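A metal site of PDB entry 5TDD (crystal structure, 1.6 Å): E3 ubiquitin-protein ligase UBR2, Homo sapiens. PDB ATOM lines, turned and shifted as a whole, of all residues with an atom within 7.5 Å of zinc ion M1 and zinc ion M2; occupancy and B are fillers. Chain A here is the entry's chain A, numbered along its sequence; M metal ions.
The side-chain sulfur of Cys 71 lies close to the backbone NH of Lys 73. N of Cys 7 lies within hydrogen-bond range of O of Cys 59. The side-chain sulfur (SG) of Cys 7 lies close to the backbone NH (N) of Arg 9 (3.6 Å). N of Cys 57 sits at hydrogen-bond distance from O of Arg 9, 2.8 Å away. O of His 74 lies within hydrogen-bond range of N of Ser 5, at 3.0 Å. SG of Cys 57 sits close to N of Cys 59 (3.4 Å).
Zinc ion M1 is bound by a ring nitrogen (ND1) of His 74 (2.1 Å), the side-chain sulfur of Cys 71 (2.3 Å), the side-chain sulfur of Cys 59 (2.3 Å) and the side-chain sulfur of Cys 35 (2.4 Å). Zinc ion M1 has four donor atoms within binding distance.
The nearest printed residue that does not touch zinc ion M2 is Cys 59 (4.2 Å).
Within 4 Å of zinc ion M1: Cys 35, Cys 59, Cys 71 and His 74. The nearest printed residue that does not touch zinc ion M1 is Cys 7 (4.4 Å).
SG of Cys 7 binds zinc ion M2, 2.3 Å away. SG of Cys 32 binds zinc ion M2 (2.4 Å). SG of Cys 57 is bound to zinc ion M2 (2.4 Å). The side-chain sulfur (SG) of Cys 35 is bound to zinc ion M2 (2.4 Å). Zinc ion M2 has four donor atoms within binding distance.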
ATOM      1  N   SER A   5     -35.534 -16.844  21.308  1.00  0.00           N
ATOM      2  CA  SER A   5     -35.231 -15.720  22.186  1.00  0.00           C
ATOM      3  C   SER A   5     -33.742 -15.715  22.535  1.00  0.00           C
ATOM      4  O   SER A   5     -33.049 -16.730  22.413  1.00  0.00           O
ATOM      5  CB  SER A   5     -36.083 -15.741  23.458  1.00  0.00           C
ATOM      6  OG  SER A   5     -35.886 -16.939  24.197  1.00  0.00           O
ATOM      7  N   LEU A   6     -33.274 -14.556  23.006  1.00  0.00           N
ATOM      8  CA  LEU A   6     -31.912 -14.366  23.476  1.00  0.00           C
ATOM      9  C   LEU A   6     -31.844 -14.518  24.992  1.00  0.00           C
ATOM     10  O   LEU A   6     -32.720 -14.042  25.733  1.00  0.00           O
ATOM     11  CB  LEU A   6     -31.382 -12.977  23.086  1.00  0.00           C
ATOM     12  CG  LEU A   6     -31.232 -12.682  21.592  1.00  0.00           C
ATOM     13  CD1 LEU A   6     -31.157 -11.178  21.394  1.00  0.00           C
ATOM     14  CD2 LEU A   6     -29.998 -13.309  21.055  1.00  0.00           C
ATOM     15  N   CYS A   7     -30.787 -15.169  25.472  1.00  0.00           N
ATOM     16  CA  CYS A   7     -30.551 -15.247  26.907  1.00  0.00           C
ATOM     17  C   CYS A   7     -30.064 -13.919  27.453  1.00  0.00           C
ATOM     18  O   CYS A   7     -30.685 -13.346  28.348  1.00  0.00           O
ATOM     19  CB  CYS A   7     -29.544 -16.344  27.218  1.00  0.00           C
ATOM     20  SG  CYS A   7     -29.119 -16.458  29.025  1.00  0.00           S
ATOM     21  N   GLY A   8     -28.908 -13.460  26.987  1.00  0.00           N
ATOM     22  CA  GLY A   8     -28.352 -12.192  27.401  1.00  0.00           C
ATOM     23  C   GLY A   8     -27.791 -12.087  28.811  1.00  0.00           C
ATOM     24  O   GLY A   8     -27.411 -10.978  29.213  1.00  0.00           O
ATOM     25  N   ARG A   9     -27.732 -13.183  29.563  1.00  0.00           N
ATOM     26  CA  ARG A   9     -27.246 -13.160  30.934  1.00  0.00           C
ATOM     27  C   ARG A   9     -25.822 -12.605  31.023  1.00  0.00           C
ATOM     28  O   ARG A   9     -24.936 -13.084  30.323  1.00  0.00           O
ATOM     29  CB  ARG A   9     -27.251 -14.569  31.524  1.00  0.00           C
ATOM     30  CG  ARG A   9     -26.686 -14.651  32.888  1.00  0.00           C
ATOM     31  CD  ARG A   9     -26.663 -16.036  33.480  1.00  0.00           C
ATOM     32  NE  ARG A   9     -25.870 -16.034  34.704  1.00  0.00           N
ATOM     33  CZ  ARG A   9     -26.311 -15.606  35.885  1.00  0.00           C
ATOM     34  NH1 ARG A   9     -27.567 -15.169  36.025  1.00  0.00           N
ATOM     35  NH2 ARG A   9     -25.498 -15.646  36.940  1.00  0.00           N
ATOM     36  N   PHE A  11     -22.433 -12.358  33.128  1.00  0.00           N
ATOM     37  CA  PHE A  11     -21.794 -13.297  34.022  1.00  0.00           C
ATOM     38  C   PHE A  11     -21.278 -12.605  35.279  1.00  0.00           C
ATOM     39  O   PHE A  11     -20.793 -11.468  35.253  1.00  0.00           O
ATOM     40  CB  PHE A  11     -20.635 -14.014  33.343  1.00  0.00           C
ATOM     41  CG  PHE A  11     -21.028 -14.770  32.101  1.00  0.00           C
ATOM     42  CD1 PHE A  11     -21.887 -15.844  32.170  1.00  0.00           C
ATOM     43  CD2 PHE A  11     -20.499 -14.428  30.872  1.00  0.00           C
ATOM     44  CE1 PHE A  11     -22.221 -16.555  31.026  1.00  0.00           C
ATOM     45  CE2 PHE A  11     -20.829 -15.140  29.742  1.00  0.00           C
ATOM     46  CZ  PHE A  11     -21.687 -16.190  29.805  1.00  0.00           C
ATOM     47  N   GLU A  15     -17.879 -17.024  37.472  1.00  0.00           N
ATOM     48  CA  GLU A  15     -18.923 -17.884  36.902  1.00  0.00           C
ATOM     49  C   GLU A  15     -18.395 -18.672  35.706  1.00  0.00           C
ATOM     50  O   GLU A  15     -17.764 -18.084  34.822  1.00  0.00           O
ATOM     51  CB  GLU A  15     -20.121 -17.046  36.458  1.00  0.00           C
ATOM     52  CG  GLU A  15     -21.277 -17.855  35.892  1.00  0.00           C
ATOM     53  CD  GLU A  15     -22.552 -17.063  35.648  1.00  0.00           C
ATOM     54  OE1 GLU A  15     -22.659 -15.927  36.156  1.00  0.00           O
ATOM     55  OE2 GLU A  15     -23.460 -17.595  34.931  1.00  0.00           O
ATOM     56  N   VAL A  30     -19.981 -17.880  23.903  1.00  0.00           N
ATOM     57  CA  VAL A  30     -20.126 -18.688  25.112  1.00  0.00           C
ATOM     58  C   VAL A  30     -21.589 -18.783  25.540  1.00  0.00           C
ATOM     59  O   VAL A  30     -22.430 -17.973  25.164  1.00  0.00           O
ATOM     60  CB  VAL A  30     -19.285 -18.147  26.302  1.00  0.00           C
ATOM     61  CG1 VAL A  30     -17.796 -18.383  26.075  1.00  0.00           C
ATOM     62  CG2 VAL A  30     -19.573 -16.700  26.508  1.00  0.00           C
ATOM     63  N   LEU A  31     -21.851 -19.788  26.376  1.00  0.00           N
ATOM     64  CA  LEU A  31     -23.146 -20.020  26.998  1.00  0.00           C
ATOM     65  C   LEU A  31     -22.992 -20.074  28.514  1.00  0.00           C
ATOM     66  O   LEU A  31     -21.980 -20.546  29.036  1.00  0.00           O
ATOM     67  CB  LEU A  31     -23.762 -21.345  26.544  1.00  0.00           C
ATOM     68  CG  LEU A  31     -23.907 -21.542  25.049  1.00  0.00           C
ATOM     69  CD1 LEU A  31     -24.271 -22.991  24.754  1.00  0.00           C
ATOM     70  CD2 LEU A  31     -24.983 -20.595  24.503  1.00  0.00           C
ATOM     71  N   CYS A  32     -23.970 -19.548  29.219  1.00  0.00           N
ATOM     72  CA  CYS A  32     -24.066 -19.782  30.646  1.00  0.00           C
ATOM     73  C   CYS A  32     -24.329 -21.267  30.908  1.00  0.00           C
ATOM     74  O   CYS A  32     -24.733 -22.016  30.014  1.00  0.00           O
ATOM     75  CB  CYS A  32     -25.168 -18.906  31.265  1.00  0.00           C
ATOM     76  SG  CYS A  32     -26.906 -19.348  30.798  1.00  0.00           S
ATOM     77  N   MET A  33     -24.118 -21.699  32.152  1.00  0.00           N
ATOM     78  CA  MET A  33     -24.238 -23.136  32.425  1.00  0.00           C
ATOM     79  C   MET A  33     -25.642 -23.650  32.159  1.00  0.00           C
ATOM     80  O   MET A  33     -25.791 -24.751  31.618  1.00  0.00           O
ATOM     81  CB  MET A  33     -23.817 -23.458  33.851  1.00  0.00           C
ATOM     82  CG  MET A  33     -23.661 -25.009  34.065  1.00  0.00           C
ATOM     83  SD  MET A  33     -23.258 -25.382  35.770  1.00  0.00           S
ATOM     84  CE  MET A  33     -21.637 -24.660  35.923  1.00  0.00           C
ATOM     85  N   GLU A  34     -26.686 -22.879  32.506  1.00  0.00           N
ATOM     86  CA  GLU A  34     -28.055 -23.329  32.265  1.00  0.00           C
ATOM     87  C   GLU A  34     -28.315 -23.563  30.790  1.00  0.00           C
ATOM     88  O   GLU A  34     -28.891 -24.585  30.401  1.00  0.00           O
ATOM     89  CB  GLU A  34     -29.055 -22.320  32.825  1.00  0.00           C
ATOM     90  CG  GLU A  34     -30.494 -22.725  32.621  1.00  0.00           C
ATOM     91  CD  GLU A  34     -31.479 -21.798  33.316  1.00  0.00           C
ATOM     92  OE1 GLU A  34     -31.119 -20.635  33.626  1.00  0.00           O
ATOM     93  OE2 GLU A  34     -32.613 -22.264  33.549  1.00  0.00           O
ATOM     94  N   CYS A  35     -27.889 -22.625  29.951  1.00  0.00           N
ATOM     95  CA  CYS A  35     -28.109 -22.772  28.508  1.00  0.00           C
ATOM     96  C   CYS A  35     -27.262 -23.912  27.956  1.00  0.00           C
ATOM     97  O   CYS A  35     -27.752 -24.734  27.166  1.00  0.00           O
ATOM     98  CB  CYS A  35     -27.797 -21.458  27.802  1.00  0.00           C
ATOM     99  SG  CYS A  35     -28.998 -20.144  28.160  1.00  0.00           S
ATOM    100  N   PHE A  36     -26.006 -23.999  28.409  1.00  0.00           N
ATOM    101  CA  PHE A  36     -25.132 -25.086  27.992  1.00  0.00           C
ATOM    102  C   PHE A  36     -25.775 -26.441  28.261  1.00  0.00           C
ATOM    103  O   PHE A  36     -25.823 -27.305  27.368  1.00  0.00           O
ATOM    104  CB  PHE A  36     -23.782 -24.976  28.745  1.00  0.00           C
ATOM    105  CG  PHE A  36     -22.899 -26.167  28.567  1.00  0.00           C
ATOM    106  CD1 PHE A  36     -22.351 -26.473  27.331  1.00  0.00           C
ATOM    107  CD2 PHE A  36     -22.610 -26.997  29.648  1.00  0.00           C
ATOM    108  CE1 PHE A  36     -21.555 -27.577  27.169  1.00  0.00           C
ATOM    109  CE2 PHE A  36     -21.810 -28.078  29.494  1.00  0.00           C
ATOM    110  CZ  PHE A  36     -21.276 -28.368  28.256  1.00  0.00           C
ATOM    111  N   GLY A  38     -28.796 -27.230  28.646  1.00  0.00           N
ATOM    112  CA  GLY A  38     -29.977 -27.382  27.817  1.00  0.00           C
ATOM    113  C   GLY A  38     -29.736 -27.366  26.313  1.00  0.00           C
ATOM    114  O   GLY A  38     -30.693 -27.285  25.534  1.00  0.00           O
ATOM    115  N   SER A  39     -28.487 -27.439  25.883  1.00  0.00           N
ATOM    116  CA  SER A  39     -28.117 -27.286  24.481  1.00  0.00           C
ATOM    117  C   SER A  39     -27.513 -28.578  23.921  1.00  0.00           C
ATOM    118  O   SER A  39     -27.063 -29.465  24.648  1.00  0.00           O
ATOM    119  CB  SER A  39     -27.112 -26.160  24.307  1.00  0.00           C
ATOM    120  OG  SER A  39     -25.792 -26.560  24.615  1.00  0.00           O
ATOM    121  N   PHE A  56     -21.228 -11.897  28.511  1.00  0.00           N
ATOM    122  CA  PHE A  56     -22.631 -12.301  28.496  1.00  0.00           C
ATOM    123  C   PHE A  56     -22.867 -13.531  27.622  1.00  0.00           C
ATOM    124  O   PHE A  56     -22.091 -13.858  26.729  1.00  0.00           O
ATOM    125  CB  PHE A  56     -23.562 -11.132  28.091  1.00  0.00           C
ATOM    126  CG  PHE A  56     -23.399 -10.699  26.671  1.00  0.00           C
ATOM    127  CD1 PHE A  56     -22.474  -9.711  26.322  1.00  0.00           C
ATOM    128  CD2 PHE A  56     -24.190 -11.256  25.672  1.00  0.00           C
ATOM    129  CE1 PHE A  56     -22.327  -9.303  24.984  1.00  0.00           C
ATOM    130  CE2 PHE A  56     -24.045 -10.855  24.341  1.00  0.00           C
ATOM    131  CZ  PHE A  56     -23.129  -9.885  24.001  1.00  0.00           C
ATOM    132  N   CYS A  57     -23.941 -14.240  27.951  1.00  0.00           N
ATOM    133  CA  CYS A  57     -24.330 -15.455  27.257  1.00  0.00           C
ATOM    134  C   CYS A  57     -24.849 -15.157  25.840  1.00  0.00           C
ATOM    135  O   CYS A  57     -25.682 -14.264  25.636  1.00  0.00           O
ATOM    136  CB  CYS A  57     -25.432 -16.137  28.071  1.00  0.00           C
ATOM    137  SG  CYS A  57     -26.029 -17.687  27.308  1.00  0.00           S
ATOM    138  N   ASP A  58     -24.377 -15.952  24.870  1.00  0.00           N
ATOM    139  CA  ASP A  58     -24.746 -15.785  23.455  1.00  0.00           C
ATOM    140  C   ASP A  58     -25.822 -16.758  23.009  1.00  0.00           C
ATOM    141  O   ASP A  58     -26.008 -16.950  21.811  1.00  0.00           O
ATOM    142  CB  ASP A  58     -23.500 -15.948  22.571  1.00  0.00           C
ATOM    143  CG  ASP A  58     -22.408 -14.950  22.935  1.00  0.00           C
ATOM    144  OD1 ASP A  58     -22.693 -13.733  22.865  1.00  0.00           O
ATOM    145  OD2 ASP A  58     -21.276 -15.373  23.312  1.00  0.00           O
ATOM    146  N   CYS A  59     -26.559 -17.368  23.955  1.00  0.00           N
ATOM    147  CA  CYS A  59     -27.637 -18.253  23.560  1.00  0.00           C
ATOM    148  C   CYS A  59     -28.695 -17.458  22.784  1.00  0.00           C
ATOM    149  O   CYS A  59     -29.100 -16.363  23.205  1.00  0.00           O
ATOM    150  CB  CYS A  59     -28.225 -18.924  24.793  1.00  0.00           C
ATOM    151  SG  CYS A  59     -29.382 -20.245  24.354  1.00  0.00           S
ATOM    152  N   GLY A  60     -29.142 -18.008  21.661  1.00  0.00           N
ATOM    153  CA  GLY A  60     -30.120 -17.350  20.795  1.00  0.00           C
ATOM    154  C   GLY A  60     -29.536 -16.494  19.688  1.00  0.00           C
ATOM    155  O   GLY A  60     -30.285 -16.033  18.813  1.00  0.00           O
ATOM    156  N   PRO A  69     -27.987 -22.762  17.937  1.00  0.00           N
ATOM    157  CA  PRO A  69     -27.884 -21.446  18.567  1.00  0.00           C
ATOM    158  C   PRO A  69     -28.749 -21.288  19.792  1.00  0.00           C
ATOM    159  O   PRO A  69     -28.470 -20.403  20.597  1.00  0.00           O
ATOM    160  CB  PRO A  69     -28.304 -20.463  17.466  1.00  0.00           C
ATOM    161  CG  PRO A  69     -29.199 -21.285  16.626  1.00  0.00           C
ATOM    162  CD  PRO A  69     -28.651 -22.674  16.636  1.00  0.00           C
ATOM    163  N   TYR A  70     -29.782 -22.108  19.962  1.00  0.00           N
ATOM    164  CA  TYR A  70     -30.700 -22.009  21.093  1.00  0.00           C
ATOM    165  C   TYR A  70     -30.589 -23.243  21.982  1.00  0.00           C
ATOM    166  O   TYR A  70     -30.258 -24.327  21.538  1.00  0.00           O
ATOM    167  CB  TYR A  70     -32.179 -21.897  20.619  1.00  0.00           C
ATOM    168  CG  TYR A  70     -32.512 -20.737  19.715  1.00  0.00           C
ATOM    169  CD1 TYR A  70     -32.498 -20.880  18.352  1.00  0.00           C
ATOM    170  CD2 TYR A  70     -32.852 -19.499  20.255  1.00  0.00           C
ATOM    171  CE1 TYR A  70     -32.788 -19.799  17.511  1.00  0.00           C
ATOM    172  CE2 TYR A  70     -33.153 -18.403  19.425  1.00  0.00           C
ATOM    173  CZ  TYR A  70     -33.116 -18.568  18.062  1.00  0.00           C
ATOM    174  OH  TYR A  70     -33.403 -17.488  17.235  1.00  0.00           O
ATOM    175  N   CYS A  71     -30.968 -23.062  23.230  1.00  0.00           N
ATOM    176  CA  CYS A  71     -31.113 -24.153  24.182  1.00  0.00           C
ATOM    177  C   CYS A  71     -32.607 -24.444  24.397  1.00  0.00           C
ATOM    178  O   CYS A  71     -33.490 -23.761  23.867  1.00  0.00           O
ATOM    179  CB  CYS A  71     -30.433 -23.819  25.514  1.00  0.00           C
ATOM    180  SG  CYS A  71     -31.396 -22.642  26.524  1.00  0.00           S
ATOM    181  N   GLN A  72     -32.885 -25.492  25.190  1.00  0.00           N
ATOM    182  CA  GLN A  72     -34.272 -25.896  25.426  1.00  0.00           C
ATOM    183  C   GLN A  72     -35.104 -24.764  26.004  1.00  0.00           C
ATOM    184  O   GLN A  72     -36.300 -24.667  25.727  1.00  0.00           O
ATOM    185  CB  GLN A  72     -34.295 -27.075  26.399  1.00  0.00           C
ATOM    186  CG  GLN A  72     -33.701 -28.327  25.844  1.00  0.00           C
ATOM    187  CD  GLN A  72     -33.893 -29.480  26.810  1.00  0.00           C
ATOM    188  OE1 GLN A  72     -33.773 -29.305  28.031  1.00  0.00           O
ATOM    189  NE2 GLN A  72     -34.222 -30.671  26.264  1.00  0.00           N
ATOM    190  N   LYS A  73     -34.491 -23.915  26.823  1.00  0.00           N
ATOM    191  CA  LYS A  73     -35.185 -22.832  27.515  1.00  0.00           C
ATOM    192  C   LYS A  73     -35.515 -21.683  26.602  1.00  0.00           C
ATOM    193  O   LYS A  73     -36.540 -21.025  26.809  1.00  0.00           O
ATOM    194  CB  LYS A  73     -34.317 -22.302  28.660  1.00  0.00           C
ATOM    195  CG  LYS A  73     -34.967 -21.171  29.476  1.00  0.00           C
ATOM    196  CD  LYS A  73     -34.102 -20.769  30.670  1.00  0.00           C
ATOM    197  CE  LYS A  73     -34.864 -19.887  31.670  1.00  0.00           C
ATOM    198  NZ  LYS A  73     -34.364 -20.083  33.093  1.00  0.00           N
ATOM    199  N   HIS A  74     -34.662 -21.410  25.613  1.00  0.00           N
ATOM    200  CA  HIS A  74     -34.810 -20.227  24.751  1.00  0.00           C
ATOM    201  C   HIS A  74     -35.319 -20.528  23.356  1.00  0.00           C
ATOM    202  O   HIS A  74     -35.667 -19.578  22.630  1.00  0.00           O
ATOM    203  CB  HIS A  74     -33.474 -19.465  24.688  1.00  0.00           C
ATOM    204  CG  HIS A  74     -33.119 -18.845  26.002  1.00  0.00           C
ATOM    205  ND1 HIS A  74     -32.040 -19.232  26.769  1.00  0.00           N
ATOM    206  CD2 HIS A  74     -33.766 -17.914  26.721  1.00  0.00           C
ATOM    207  CE1 HIS A  74     -32.039 -18.561  27.900  1.00  0.00           C
ATOM    208  NE2 HIS A  74     -33.070 -17.726  27.882  1.00  0.00           N
ATOM    209  N   GLU A  75     -35.435 -21.793  22.976  1.00  0.00           N
ATOM    210  CA  GLU A  75     -35.936 -22.160  21.661  1.00  0.00           C
ATOM    211  C   GLU A  75     -37.366 -21.689  21.526  1.00  0.00           C
ATOM    212  O   GLU A  75     -37.767 -21.382  20.395  1.00  0.00           O
ATOM    213  CB  GLU A  75     -35.829 -23.682  21.422  1.00  0.00           C
ATOM    214  CG  GLU A  75     -36.800 -24.542  22.233  1.00  0.00           C
ATOM    215  CD  GLU A  75     -36.527 -26.044  22.055  1.00  0.00           C
ATOM    216  OE1 GLU A  75     -36.138 -26.404  20.922  1.00  0.00           O
ATOM    217  OE2 GLU A  75     -36.700 -26.846  23.001  1.00  0.00           O
HETATM  218 ZN    ZN M   1     -30.488 -20.529  26.366  1.00  0.00          ZN
HETATM  219 ZN    ZN M   2     -27.695 -18.272  28.862  1.00  0.00          ZN
